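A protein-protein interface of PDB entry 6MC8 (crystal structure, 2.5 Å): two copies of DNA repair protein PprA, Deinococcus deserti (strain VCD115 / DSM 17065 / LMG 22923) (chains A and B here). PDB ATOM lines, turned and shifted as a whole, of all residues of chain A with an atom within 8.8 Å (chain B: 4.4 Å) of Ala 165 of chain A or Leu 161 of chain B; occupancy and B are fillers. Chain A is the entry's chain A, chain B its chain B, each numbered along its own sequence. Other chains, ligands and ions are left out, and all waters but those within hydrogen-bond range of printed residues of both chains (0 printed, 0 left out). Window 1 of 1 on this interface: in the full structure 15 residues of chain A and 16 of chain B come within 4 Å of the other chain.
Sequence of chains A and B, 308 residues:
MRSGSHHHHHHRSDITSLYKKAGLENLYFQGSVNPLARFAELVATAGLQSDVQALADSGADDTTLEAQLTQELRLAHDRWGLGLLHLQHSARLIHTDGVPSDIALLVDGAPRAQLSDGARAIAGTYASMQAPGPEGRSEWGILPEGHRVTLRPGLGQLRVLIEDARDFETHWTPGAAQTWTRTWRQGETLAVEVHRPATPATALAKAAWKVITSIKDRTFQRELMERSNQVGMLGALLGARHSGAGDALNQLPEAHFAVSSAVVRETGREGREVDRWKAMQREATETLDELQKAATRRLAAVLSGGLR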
ATOM      1  N   HIS A 147       1.913  -3.091   5.743  1.00  0.00           N
ATOM      2  CA  HIS A 147       2.471  -4.304   5.169  1.00  0.00           C
ATOM      3  C   HIS A 147       1.416  -5.399   5.126  1.00  0.00           C
ATOM      4  O   HIS A 147       0.844  -5.761   6.157  1.00  0.00           O
ATOM      5  CB  HIS A 147       3.676  -4.767   5.974  1.00  0.00           C
ATOM      6  CG  HIS A 147       4.333  -5.989   5.420  1.00  0.00           C
ATOM      7  ND1 HIS A 147       5.153  -5.955   4.314  1.00  0.00           N
ATOM      8  CD2 HIS A 147       4.271  -7.285   5.801  1.00  0.00           C
ATOM      9  CE1 HIS A 147       5.582  -7.174   4.050  1.00  0.00           C
ATOM     10  NE2 HIS A 147       5.059  -8.001   4.936  1.00  0.00           N
ATOM     11  N   VAL A 149       0.865  -9.462   3.965  1.00  0.00           N
ATOM     12  CA  VAL A 149       1.718 -10.642   3.902  1.00  0.00           C
ATOM     13  C   VAL A 149       1.508 -11.346   2.570  1.00  0.00           C
ATOM     14  O   VAL A 149       0.372 -11.613   2.167  1.00  0.00           O
ATOM     15  CB  VAL A 149       1.417 -11.588   5.076  1.00  0.00           C
ATOM     16  CG1 VAL A 149       2.307 -12.822   5.033  1.00  0.00           C
ATOM     17  CG2 VAL A 149       1.566 -10.864   6.384  1.00  0.00           C
ATOM     18  N   GLY A 156       3.558 -21.784   8.457  1.00  0.00           N
ATOM     19  CA  GLY A 156       4.456 -21.278   9.481  1.00  0.00           C
ATOM     20  C   GLY A 156       4.402 -19.771   9.621  1.00  0.00           C
ATOM     21  O   GLY A 156       4.639 -19.229  10.704  1.00  0.00           O
ATOM     22  N   GLN A 157       4.120 -19.072   8.519  1.00  0.00           N
ATOM     23  CA  GLN A 157       3.852 -17.639   8.593  1.00  0.00           C
ATOM     24  C   GLN A 157       2.595 -17.352   9.402  1.00  0.00           C
ATOM     25  O   GLN A 157       2.604 -16.496  10.290  1.00  0.00           O
ATOM     26  CB  GLN A 157       3.728 -17.046   7.192  1.00  0.00           C
ATOM     27  CG  GLN A 157       5.031 -16.672   6.524  1.00  0.00           C
ATOM     28  CD  GLN A 157       4.836 -16.267   5.082  1.00  0.00           C
ATOM     29  OE1 GLN A 157       3.824 -16.582   4.482  1.00  0.00           O
ATOM     30  NE2 GLN A 157       5.767 -15.504   4.549  1.00  0.00           N
ATOM     31  N   LEU A 158       1.513 -18.077   9.124  1.00  0.00           N
ATOM     32  CA  LEU A 158       0.242 -17.814   9.790  1.00  0.00           C
ATOM     33  C   LEU A 158       0.273 -18.226  11.252  1.00  0.00           C
ATOM     34  O   LEU A 158      -0.460 -17.663  12.066  1.00  0.00           O
ATOM     35  CB  LEU A 158      -0.890 -18.532   9.061  1.00  0.00           C
ATOM     36  CG  LEU A 158      -1.252 -17.948   7.703  1.00  0.00           C
ATOM     37  CD1 LEU A 158      -2.190 -18.864   6.961  1.00  0.00           C
ATOM     38  CD2 LEU A 158      -1.887 -16.588   7.900  1.00  0.00           C
ATOM     39  N   ARG A 159       1.117 -19.194  11.607  1.00  0.00           N
ATOM     40  CA  ARG A 159       1.173 -19.659  12.988  1.00  0.00           C
ATOM     41  C   ARG A 159       1.768 -18.599  13.905  1.00  0.00           C
ATOM     42  O   ARG A 159       1.301 -18.401  15.028  1.00  0.00           O
ATOM     43  CB  ARG A 159       1.967 -20.961  13.068  1.00  0.00           C
ATOM     44  CG  ARG A 159       2.020 -21.573  14.448  1.00  0.00           C
ATOM     45  CD  ARG A 159       2.660 -22.937  14.409  1.00  0.00           C
ATOM     46  NE  ARG A 159       1.817 -23.893  13.702  1.00  0.00           N
ATOM     47  CZ  ARG A 159       0.828 -24.574  14.271  1.00  0.00           C
ATOM     48  NH1 ARG A 159       0.570 -24.412  15.560  1.00  0.00           N
ATOM     49  NH2 ARG A 159       0.106 -25.425  13.558  1.00  0.00           N
ATOM     50  N   VAL A 160       2.779 -17.879  13.425  1.00  0.00           N
ATOM     51  CA  VAL A 160       3.387 -16.832  14.236  1.00  0.00           C
ATOM     52  C   VAL A 160       2.508 -15.584  14.245  1.00  0.00           C
ATOM     53  O   VAL A 160       2.403 -14.891  15.263  1.00  0.00           O
ATOM     54  CB  VAL A 160       4.812 -16.548  13.726  1.00  0.00           C
ATOM     55  CG1 VAL A 160       5.487 -15.461  14.533  1.00  0.00           C
ATOM     56  CG2 VAL A 160       5.642 -17.811  13.755  1.00  0.00           C
ATOM     57  N   LEU A 161       1.837 -15.299  13.128  1.00  0.00           N
ATOM     58  CA  LEU A 161       0.983 -14.115  13.045  1.00  0.00           C
ATOM     59  C   LEU A 161      -0.263 -14.259  13.914  1.00  0.00           C
ATOM     60  O   LEU A 161      -0.737 -13.284  14.505  1.00  0.00           O
ATOM     61  CB  LEU A 161       0.598 -13.853  11.589  1.00  0.00           C
ATOM     62  CG  LEU A 161       1.686 -13.390  10.620  1.00  0.00           C
ATOM     63  CD1 LEU A 161       1.187 -13.470   9.197  1.00  0.00           C
ATOM     64  CD2 LEU A 161       2.138 -11.988  10.932  1.00  0.00           C
ATOM     65  N   ILE A 162      -0.803 -15.472  14.011  1.00  0.00           N
ATOM     66  CA  ILE A 162      -1.993 -15.694  14.826  1.00  0.00           C
ATOM     67  C   ILE A 162      -1.624 -15.756  16.305  1.00  0.00           C
ATOM     68  O   ILE A 162      -2.249 -15.094  17.141  1.00  0.00           O
ATOM     69  CB  ILE A 162      -2.729 -16.963  14.356  1.00  0.00           C
ATOM     70  CG1 ILE A 162      -3.386 -16.731  12.997  1.00  0.00           C
ATOM     71  CG2 ILE A 162      -3.780 -17.391  15.333  1.00  0.00           C
ATOM     72  CD1 ILE A 162      -3.834 -17.996  12.326  1.00  0.00           C
ATOM     73  N   GLU A 163      -0.589 -16.526  16.646  1.00  0.00           N
ATOM     74  CA  GLU A 163      -0.232 -16.726  18.049  1.00  0.00           C
ATOM     75  C   GLU A 163       0.423 -15.489  18.651  1.00  0.00           C
ATOM     76  O   GLU A 163       0.058 -15.054  19.748  1.00  0.00           O
ATOM     77  CB  GLU A 163       0.705 -17.923  18.195  1.00  0.00           C
ATOM     78  CG  GLU A 163       0.073 -19.274  17.980  1.00  0.00           C
ATOM     79  CD  GLU A 163       1.081 -20.396  18.069  1.00  0.00           C
ATOM     80  OE1 GLU A 163       2.291 -20.107  18.092  1.00  0.00           O
ATOM     81  OE2 GLU A 163       0.667 -21.566  18.135  1.00  0.00           O
ATOM     82  N   ASP A 164       1.395 -14.914  17.951  1.00  0.00           N
ATOM     83  CA  ASP A 164       2.339 -13.993  18.560  1.00  0.00           C
ATOM     84  C   ASP A 164       2.159 -12.545  18.137  1.00  0.00           C
ATOM     85  O   ASP A 164       2.614 -11.649  18.848  1.00  0.00           O
ATOM     86  CB  ASP A 164       3.770 -14.433  18.232  1.00  0.00           C
ATOM     87  CG  ASP A 164       4.092 -15.800  18.773  1.00  0.00           C
ATOM     88  OD1 ASP A 164       3.553 -16.164  19.834  1.00  0.00           O
ATOM     89  OD2 ASP A 164       4.865 -16.525  18.120  1.00  0.00           O
ATOM     90  N   ALA A 165       1.515 -12.284  17.013  1.00  0.00           N
ATOM     91  CA  ALA A 165       1.497 -10.927  16.503  1.00  0.00           C
ATOM     92  C   ALA A 165       0.257 -10.168  16.961  1.00  0.00           C
ATOM     93  O   ALA A 165      -0.703 -10.726  17.491  1.00  0.00           O
ATOM     94  CB  ALA A 165       1.578 -10.931  14.978  1.00  0.00           C
ATOM     95  N   ARG A 166       0.314  -8.861  16.748  1.00  0.00           N
ATOM     96  CA  ARG A 166      -0.797  -7.925  16.842  1.00  0.00           C
ATOM     97  C   ARG A 166      -1.472  -7.873  15.478  1.00  0.00           C
ATOM     98  O   ARG A 166      -1.562  -8.914  14.821  1.00  0.00           O
ATOM     99  CB  ARG A 166      -0.310  -6.565  17.322  1.00  0.00           C
ATOM    100  CG  ARG A 166       0.213  -6.622  18.745  1.00  0.00           C
ATOM    101  CD  ARG A 166       0.967  -5.379  19.134  1.00  0.00           C
ATOM    102  NE  ARG A 166       1.570  -5.508  20.456  1.00  0.00           N
ATOM    103  CZ  ARG A 166       1.073  -4.982  21.566  1.00  0.00           C
ATOM    104  NH1 ARG A 166      -0.020  -4.243  21.520  1.00  0.00           N
ATOM    105  NH2 ARG A 166       1.693  -5.166  22.719  1.00  0.00           N
ATOM    106  N   ASP A 167      -2.092  -6.740  15.139  1.00  0.00           N
ATOM    107  CA  ASP A 167      -2.732  -6.549  13.839  1.00  0.00           C
ATOM    108  C   ASP A 167      -1.831  -6.954  12.677  1.00  0.00           C
ATOM    109  O   ASP A 167      -0.672  -6.548  12.593  1.00  0.00           O
ATOM    110  CB  ASP A 167      -3.144  -5.091  13.640  1.00  0.00           C
ATOM    111  CG  ASP A 167      -4.146  -4.618  14.659  1.00  0.00           C
ATOM    112  OD1 ASP A 167      -4.754  -5.459  15.343  1.00  0.00           O
ATOM    113  OD2 ASP A 167      -4.362  -3.394  14.738  1.00  0.00           O
ATOM    114  N   PHE A 168      -2.365  -7.800  11.802  1.00  0.00           N
ATOM    115  CA  PHE A 168      -1.677  -8.226  10.596  1.00  0.00           C
ATOM    116  C   PHE A 168      -2.733  -8.419   9.519  1.00  0.00           C
ATOM    117  O   PHE A 168      -3.926  -8.450   9.813  1.00  0.00           O
ATOM    118  CB  PHE A 168      -0.866  -9.519  10.815  1.00  0.00           C
ATOM    119  CG  PHE A 168      -1.707 -10.758  10.976  1.00  0.00           C
ATOM    120  CD1 PHE A 168      -2.259 -11.083  12.200  1.00  0.00           C
ATOM    121  CD2 PHE A 168      -1.907 -11.626   9.909  1.00  0.00           C
ATOM    122  CE1 PHE A 168      -3.027 -12.225  12.344  1.00  0.00           C
ATOM    123  CE2 PHE A 168      -2.674 -12.757  10.054  1.00  0.00           C
ATOM    124  CZ  PHE A 168      -3.230 -13.058  11.273  1.00  0.00           C
ATOM    125  N   GLU A 169      -2.298  -8.517   8.274  1.00  0.00           N
ATOM    126  CA  GLU A 169      -3.297  -8.761   7.213  1.00  0.00           C
ATOM    127  C   GLU A 169      -2.589  -9.494   6.093  1.00  0.00           C
ATOM    128  O   GLU A 169      -1.520  -9.116   5.744  1.00  0.00           O
ATOM    129  CB  GLU A 169      -3.823  -7.463   6.617  1.00  0.00           C
ATOM    130  CG  GLU A 169      -4.776  -7.681   5.484  1.00  0.00           C
ATOM    131  CD  GLU A 169      -5.341  -6.412   4.921  1.00  0.00           C
ATOM    132  OE1 GLU A 169      -5.010  -5.333   5.452  1.00  0.00           O
ATOM    133  OE2 GLU A 169      -6.116  -6.493   3.948  1.00  0.00           O
ATOM    134  N   ARG A 185      -6.052  -9.710  11.439  1.00  0.00           N
ATOM    135  CA  ARG A 185      -6.397  -9.372  12.812  1.00  0.00           C
ATOM    136  C   ARG A 185      -6.511  -7.860  12.942  1.00  0.00           C
ATOM    137  O   ARG A 185      -5.656  -7.127  12.441  1.00  0.00           O
ATOM    138  CB  ARG A 185      -5.360  -9.913  13.808  1.00  0.00           C
ATOM    139  CG  ARG A 185      -5.612  -9.481  15.251  1.00  0.00           C
ATOM    140  CD  ARG A 185      -4.652 -10.073  16.258  1.00  0.00           C
ATOM    141  NE  ARG A 185      -4.918 -11.482  16.496  1.00  0.00           N
ATOM    142  CZ  ARG A 185      -4.074 -12.457  16.207  1.00  0.00           C
ATOM    143  NH1 ARG A 185      -2.897 -12.174  15.677  1.00  0.00           N
ATOM    144  NH2 ARG A 185      -4.402 -13.713  16.455  1.00  0.00           N
ATOM    145  N   GLN A 186      -7.575  -7.399  13.593  1.00  0.00           N
ATOM    146  CA  GLN A 186      -7.722  -5.997  13.958  1.00  0.00           C
ATOM    147  C   GLN A 186      -8.092  -5.938  15.432  1.00  0.00           C
ATOM    148  O   GLN A 186      -9.236  -6.217  15.800  1.00  0.00           O
ATOM    149  CB  GLN A 186      -8.770  -5.294  13.101  1.00  0.00           C
ATOM    150  CG  GLN A 186      -8.807  -3.802  13.327  1.00  0.00           C
ATOM    151  CD  GLN A 186      -9.815  -3.112  12.451  1.00  0.00           C
ATOM    152  OE1 GLN A 186     -10.561  -3.755  11.720  1.00  0.00           O
ATOM    153  NE2 GLN A 186      -9.837  -1.790  12.506  1.00  0.00           N
ATOM    154  N   GLY A 187      -7.125  -5.580  16.270  1.00  0.00           N
ATOM    155  CA  GLY A 187      -7.337  -5.547  17.700  1.00  0.00           C
ATOM    156  C   GLY A 187      -7.393  -6.929  18.307  1.00  0.00           C
ATOM    157  O   GLY A 187      -6.405  -7.665  18.283  1.00  0.00           O
ATOM    158  N   GLU A 188      -8.544  -7.295  18.857  1.00  0.00           N
ATOM    159  CA  GLU A 188      -8.744  -8.613  19.435  1.00  0.00           C
ATOM    160  C   GLU A 188      -9.442  -9.567  18.481  1.00  0.00           C
ATOM    161  O   GLU A 188      -9.632 -10.736  18.823  1.00  0.00           O
ATOM    162  CB  GLU A 188      -9.548  -8.504  20.732  1.00  0.00           C
ATOM    163  CG  GLU A 188      -8.861  -7.706  21.824  1.00  0.00           C
ATOM    164  CD  GLU A 188      -7.603  -8.370  22.333  1.00  0.00           C
ATOM    165  OE1 GLU A 188      -7.560  -9.617  22.376  1.00  0.00           O
ATOM    166  OE2 GLU A 188      -6.652  -7.642  22.684  1.00  0.00           O
ATOM    167  N   LEU A 190      -9.725 -11.800  15.258  1.00  0.00           N
ATOM    168  CA  LEU A 190      -9.169 -12.534  14.131  1.00  0.00           C
ATOM    169  C   LEU A 190     -10.274 -12.775  13.117  1.00  0.00           C
ATOM    170  O   LEU A 190     -11.404 -13.100  13.487  1.00  0.00           O
ATOM    171  CB  LEU A 190      -8.566 -13.870  14.570  1.00  0.00           C
ATOM    172  CG  LEU A 190      -7.890 -14.706  13.481  1.00  0.00           C
ATOM    173  CD1 LEU A 190      -6.651 -14.014  12.961  1.00  0.00           C
ATOM    174  CD2 LEU A 190      -7.570 -16.097  13.959  1.00  0.00           C
ATOM    175  N   GLY A 271      -8.810 -16.316  19.308  1.00  0.00           N
ATOM    176  CA  GLY A 271      -8.215 -15.535  18.208  1.00  0.00           C
ATOM    177  C   GLY A 271      -6.756 -15.842  17.982  1.00  0.00           C
ATOM    178  O   GLY A 271      -6.264 -15.521  16.939  1.00  0.00           O
ATOM    179  N   ARG A 272      -6.072 -16.350  18.994  1.00  0.00           N
ATOM    180  CA  ARG A 272      -4.631 -16.667  18.860  1.00  0.00           C
ATOM    181  C   ARG A 272      -4.364 -18.160  18.659  1.00  0.00           C
ATOM    182  O   ARG A 272      -3.213 -18.528  18.751  1.00  0.00           O
ATOM    183  CB  ARG A 272      -3.840 -16.103  20.031  1.00  0.00           C
ATOM    184  CG  ARG A 272      -3.947 -14.600  20.123  1.00  0.00           C
ATOM    185  CD  ARG A 272      -2.804 -13.914  20.798  1.00  0.00           C
ATOM    186  NE  ARG A 272      -2.998 -12.504  20.650  1.00  0.00           N
ATOM    187  CZ  ARG A 272      -2.375 -11.749  19.800  1.00  0.00           C
ATOM    188  NH1 ARG A 272      -1.467 -12.248  19.004  1.00  0.00           N
ATOM    189  NH2 ARG A 272      -2.660 -10.475  19.740  1.00  0.00           N
ATOM    190  N   VAL B 149       5.171 -11.328  22.951  1.00  0.00           N
ATOM    191  CA  VAL B 149       5.622 -12.645  22.522  1.00  0.00           C
ATOM    192  C   VAL B 149       6.520 -13.240  23.595  1.00  0.00           C
ATOM    193  O   VAL B 149       7.438 -12.578  24.091  1.00  0.00           O
ATOM    194  CB  VAL B 149       6.370 -12.549  21.183  1.00  0.00           C
ATOM    195  CG1 VAL B 149       6.704 -13.932  20.651  1.00  0.00           C
ATOM    196  CG2 VAL B 149       5.588 -11.752  20.188  1.00  0.00           C
ATOM    197  N   GLN B 157       9.987 -17.589  15.160  1.00  0.00           N
ATOM    198  CA  GLN B 157       8.982 -16.583  15.486  1.00  0.00           C
ATOM    199  C   GLN B 157       9.409 -15.198  15.022  1.00  0.00           C
ATOM    200  O   GLN B 157       8.622 -14.474  14.404  1.00  0.00           O
ATOM    201  CB  GLN B 157       8.715 -16.566  16.988  1.00  0.00           C
ATOM    202  CG  GLN B 157       7.922 -17.733  17.513  1.00  0.00           C
ATOM    203  CD  GLN B 157       7.717 -17.633  18.999  1.00  0.00           C
ATOM    204  OE1 GLN B 157       8.317 -16.797  19.650  1.00  0.00           O
ATOM    205  NE2 GLN B 157       6.833 -18.441  19.534  1.00  0.00           N
ATOM    206  N   LEU B 158      10.654 -14.815  15.312  1.00  0.00           N
ATOM    207  CA  LEU B 158      11.108 -13.464  14.996  1.00  0.00           C
ATOM    208  C   LEU B 158      11.239 -13.228  13.501  1.00  0.00           C
ATOM    209  O   LEU B 158      11.192 -12.079  13.066  1.00  0.00           O
ATOM    210  CB  LEU B 158      12.438 -13.168  15.684  1.00  0.00           C
ATOM    211  CG  LEU B 158      12.361 -12.850  17.171  1.00  0.00           C
ATOM    212  CD1 LEU B 158      13.732 -12.787  17.777  1.00  0.00           C
ATOM    213  CD2 LEU B 158      11.658 -11.529  17.352  1.00  0.00           C
ATOM    214  N   ARG B 159      11.391 -14.283  12.702  1.00  0.00           N
ATOM    215  CA  ARG B 159      11.497 -14.090  11.259  1.00  0.00           C
ATOM    216  C   ARG B 159      10.170 -13.641  10.666  1.00  0.00           C
ATOM    217  O   ARG B 159      10.131 -12.730   9.836  1.00  0.00           O
ATOM    218  CB  ARG B 159      11.984 -15.371  10.586  1.00  0.00           C
ATOM    219  CG  ARG B 159      12.255 -15.216   9.111  1.00  0.00           C
ATOM    220  CD  ARG B 159      12.836 -16.484   8.528  1.00  0.00           C
ATOM    221  NE  ARG B 159      14.137 -16.793   9.112  1.00  0.00           N
ATOM    222  CZ  ARG B 159      15.286 -16.270   8.701  1.00  0.00           C
ATOM    223  NH1 ARG B 159      15.308 -15.406   7.697  1.00  0.00           N
ATOM    224  NH2 ARG B 159      16.418 -16.613   9.298  1.00  0.00           N
ATOM    225  N   VAL B 160       9.069 -14.253  11.101  1.00  0.00           N
ATOM    226  CA  VAL B 160       7.752 -13.848  10.621  1.00  0.00           C
ATOM    227  C   VAL B 160       7.373 -12.489  11.198  1.00  0.00           C
ATOM    228  O   VAL B 160       6.784 -11.648  10.511  1.00  0.00           O
ATOM    229  CB  VAL B 160       6.717 -14.940  10.954  1.00  0.00           C
ATOM    230  CG1 VAL B 160       5.318 -14.529  10.556  1.00  0.00           C
ATOM    231  CG2 VAL B 160       7.085 -16.234  10.263  1.00  0.00           C
ATOM    232  N   LEU B 161       7.750 -12.234  12.452  1.00  0.00           N
ATOM    233  CA  LEU B 161       7.407 -10.971  13.100  1.00  0.00           C
ATOM    234  C   LEU B 161       8.157  -9.796  12.482  1.00  0.00           C
ATOM    235  O   LEU B 161       7.606  -8.698  12.346  1.00  0.00           O
ATOM    236  CB  LEU B 161       7.687 -11.067  14.598  1.00  0.00           C
ATOM    237  CG  LEU B 161       6.747 -11.949  15.414  1.00  0.00           C
ATOM    238  CD1 LEU B 161       7.299 -12.179  16.804  1.00  0.00           C
ATOM    239  CD2 LEU B 161       5.385 -11.304  15.493  1.00  0.00           C
ATOM    240  N   ILE B 162       9.413 -10.008  12.089  1.00  0.00           N
ATOM    241  CA  ILE B 162      10.178  -8.935  11.464  1.00  0.00           C
ATOM    242  C   ILE B 162       9.758  -8.745  10.010  1.00  0.00           C
ATOM    243  O   ILE B 162       9.534  -7.619   9.561  1.00  0.00           O
ATOM    244  CB  ILE B 162      11.688  -9.204  11.616  1.00  0.00           C
ATOM    245  CG1 ILE B 162      12.108  -9.003  13.072  1.00  0.00           C
ATOM    246  CG2 ILE B 162      12.516  -8.319  10.726  1.00  0.00           C
ATOM    247  CD1 ILE B 162      13.447  -9.587  13.403  1.00  0.00           C
ATOM    248  N   GLU B 163       9.593  -9.840   9.266  1.00  0.00           N
ATOM    249  CA  GLU B 163       9.286  -9.726   7.843  1.00  0.00           C
ATOM    250  C   GLU B 163       7.810  -9.436   7.588  1.00  0.00           C
ATOM    251  O   GLU B 163       7.478  -8.513   6.840  1.00  0.00           O
ATOM    252  CB  GLU B 163       9.698 -11.004   7.110  1.00  0.00           C
ATOM    253  CG  GLU B 163      11.195 -11.254   7.066  1.00  0.00           C
ATOM    254  CD  GLU B 163      11.555 -12.587   6.440  1.00  0.00           C
ATOM    255  OE1 GLU B 163      10.640 -13.382   6.154  1.00  0.00           O
ATOM    256  OE2 GLU B 163      12.759 -12.841   6.239  1.00  0.00           O
ATOM    257  N   ALA B 165       4.944  -9.258   9.978  1.00  0.00           N
ATOM    258  CA  ALA B 165       4.002  -8.651  10.896  1.00  0.00           C
ATOM    259  C   ALA B 165       4.103  -7.131  10.866  1.00  0.00           C
ATOM    260  O   ALA B 165       5.017  -6.539  10.290  1.00  0.00           O
ATOM    261  CB  ALA B 165       4.227  -9.164  12.314  1.00  0.00           C
ATOM    262  N   PHE B 168       4.577  -5.285  16.934  1.00  0.00           N
ATOM    263  CA  PHE B 168       4.629  -6.431  17.828  1.00  0.00           C
ATOM    264  C   PHE B 168       5.602  -6.091  18.946  1.00  0.00           C
ATOM    265  O   PHE B 168       6.328  -5.103  18.867  1.00  0.00           O
ATOM    266  CB  PHE B 168       5.048  -7.720  17.096  1.00  0.00           C
ATOM    267  CG  PHE B 168       6.502  -7.765  16.704  1.00  0.00           C
ATOM    268  CD1 PHE B 168       6.940  -7.147  15.550  1.00  0.00           C
ATOM    269  CD2 PHE B 168       7.420  -8.470  17.467  1.00  0.00           C
ATOM    270  CE1 PHE B 168       8.271  -7.191  15.191  1.00  0.00           C
ATOM    271  CE2 PHE B 168       8.748  -8.513  17.111  1.00  0.00           C
ATOM    272  CZ  PHE B 168       9.173  -7.877  15.970  1.00  0.00           C
ATOM    273  N   ARG B 185       8.390  -3.686  17.212  1.00  0.00           N
ATOM    274  CA  ARG B 185       8.130  -2.779  16.107  1.00  0.00           C
ATOM    275  C   ARG B 185       7.004  -1.841  16.503  1.00  0.00           C
ATOM    276  O   ARG B 185       5.996  -2.280  17.059  1.00  0.00           O
ATOM    277  CB  ARG B 185       7.764  -3.532  14.821  1.00  0.00           C
ATOM    278  CG  ARG B 185       7.406  -2.614  13.656  1.00  0.00           C
ATOM    279  CD  ARG B 185       7.119  -3.353  12.375  1.00  0.00           C
ATOM    280  NE  ARG B 185       8.329  -3.898  11.786  1.00  0.00           N
ATOM    281  CZ  ARG B 185       8.589  -5.190  11.669  1.00  0.00           C
ATOM    282  NH1 ARG B 185       7.719  -6.088  12.100  1.00  0.00           N
ATOM    283  NH2 ARG B 185       9.723  -5.580  11.116  1.00  0.00           N
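Hydrophobic or aromatic side chains of chain B within 4 Å of the printed part of chain A: Val 149, Val 160, Leu 161 and Ala 165.
Printed residues of chain A that touch a printed residue of chain B: His 147, Gly 156, Gln 157, Val 160, Leu 161, Asp 164 and Ala 165.
Hydrophobic or aromatic side chains of chain A that line the printed part of chain B: His 147, Val 160, Leu 161 and Ala 165.
Among the printed residues, no Asp or Glu carboxylate lies within 4 Å of a Lys or Arg side-chain nitrogen of the other chain.
Among the printed residues, pairs that only touch across the chains: Gly 156 of chain A with Val 160 of chain B, Gln 157 of chain A with Val 160 of chain B, Val 160 of chain A with Gln 157 of chain B, Val 160 of chain A with Val 160 of chain B, Val 160 of chain A with Leu 161 of chain B, Leu 161 of chain A with Val 160 of chain B, Leu 161 of chain A with Ala 165 of chain B, Asp 164 of chain A with Val 149 of chain B and Ala 165 of chain A with Leu 161 of chain B.
Printed residues of chain B within 4 Å of His 147 of chain A: Glu 163.
Of the printed residues of chain B, Asp 164 of chain A touches Val 149 and Gln 157.
Ala 165 of chain A touches just one residue of chain B: Leu 161 (3.9 Å).
Of the printed residues of chain A, Val 149 of chain B touches Asp 164 (3.3 Å).
Of the printed residues of chain A, Gln 157 of chain B touches Val 160 and Asp 164.
Printed residues of chain A within 4 Å of Val 160 of chain B: Gly 156 (3.9 Å), Gln 157 (3.4 Å), Val 160 (3.7 Å) and Leu 161 (3.8 Å).
Ala 165 of chain B touches just one residue of chain A: Leu 161.
The nearest residue of chain B that does not touch Ala 165 of chain A is Ala 165 of chain B (4.2 Å).
The nearest residue of chain A that does not touch Leu 161 of chain B is Asp 164 of chain A (4.4 Å).
N of Ala 165 of chain A is in hydrogen-bond range of O of Val 160 of chain A.
The backbone carbonyl oxygen (O) of Ala 165 of chain A lies within hydrogen-bond range of the guanidinium group (NH1) of Arg 185 of chain A, at 3.2 Å.
The backbone carbonyl oxygen (O) of Ala 165 of chain A sits at hydrogen-bond distance from the guanidinium group (NH2) of Arg 272 of chain A, at 3.0 Å.
The side-chain carboxylate of Glu 163 of chain B lies within salt-bridge range of the guanidinium group of Arg 159 of chain B, 3.9 Å away.
The backbone carbonyl oxygen of Val 160 of chain B sits at hydrogen-bond distance from the backbone NH of Ala 165 of chain B (3.1 Å).
NH1 of Arg 185 of chain B is in hydrogen-bond range of O of Leu 161 of chain B.
Gln 157 of chain A touches Val 160 of chain B, and with the chains exchanged Val 160 of chain A touches Gln 157 of chain B.
Val 160 of chain A touches its own counterpart, Val 160 of chain B.
Val 160 of chain A touches Leu 161 of chain B, and with the chains exchanged Leu 161 of chain A touches Val 160 of chain B.
Leu 161 of chain A touches Ala 165 of chain B, and with the chains exchanged Ala 165 of chain A touches Leu 161 of chain B.
Of the 11 pairs that touch across the chains among the printed residues, 7 have their exchanged pair printed and touching as well.
A ring nitrogen (NE2) of His 147 of chain A sits at hydrogen-bond distance from the backbone carbonyl oxygen of Glu 163 of chain B.
The side-chain amide nitrogen (NE2) of Gln 157 of chain B lies within hydrogen-bond range of the side-chain carboxylate (OD2) of Asp 164 of chain A (3.1 Å).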
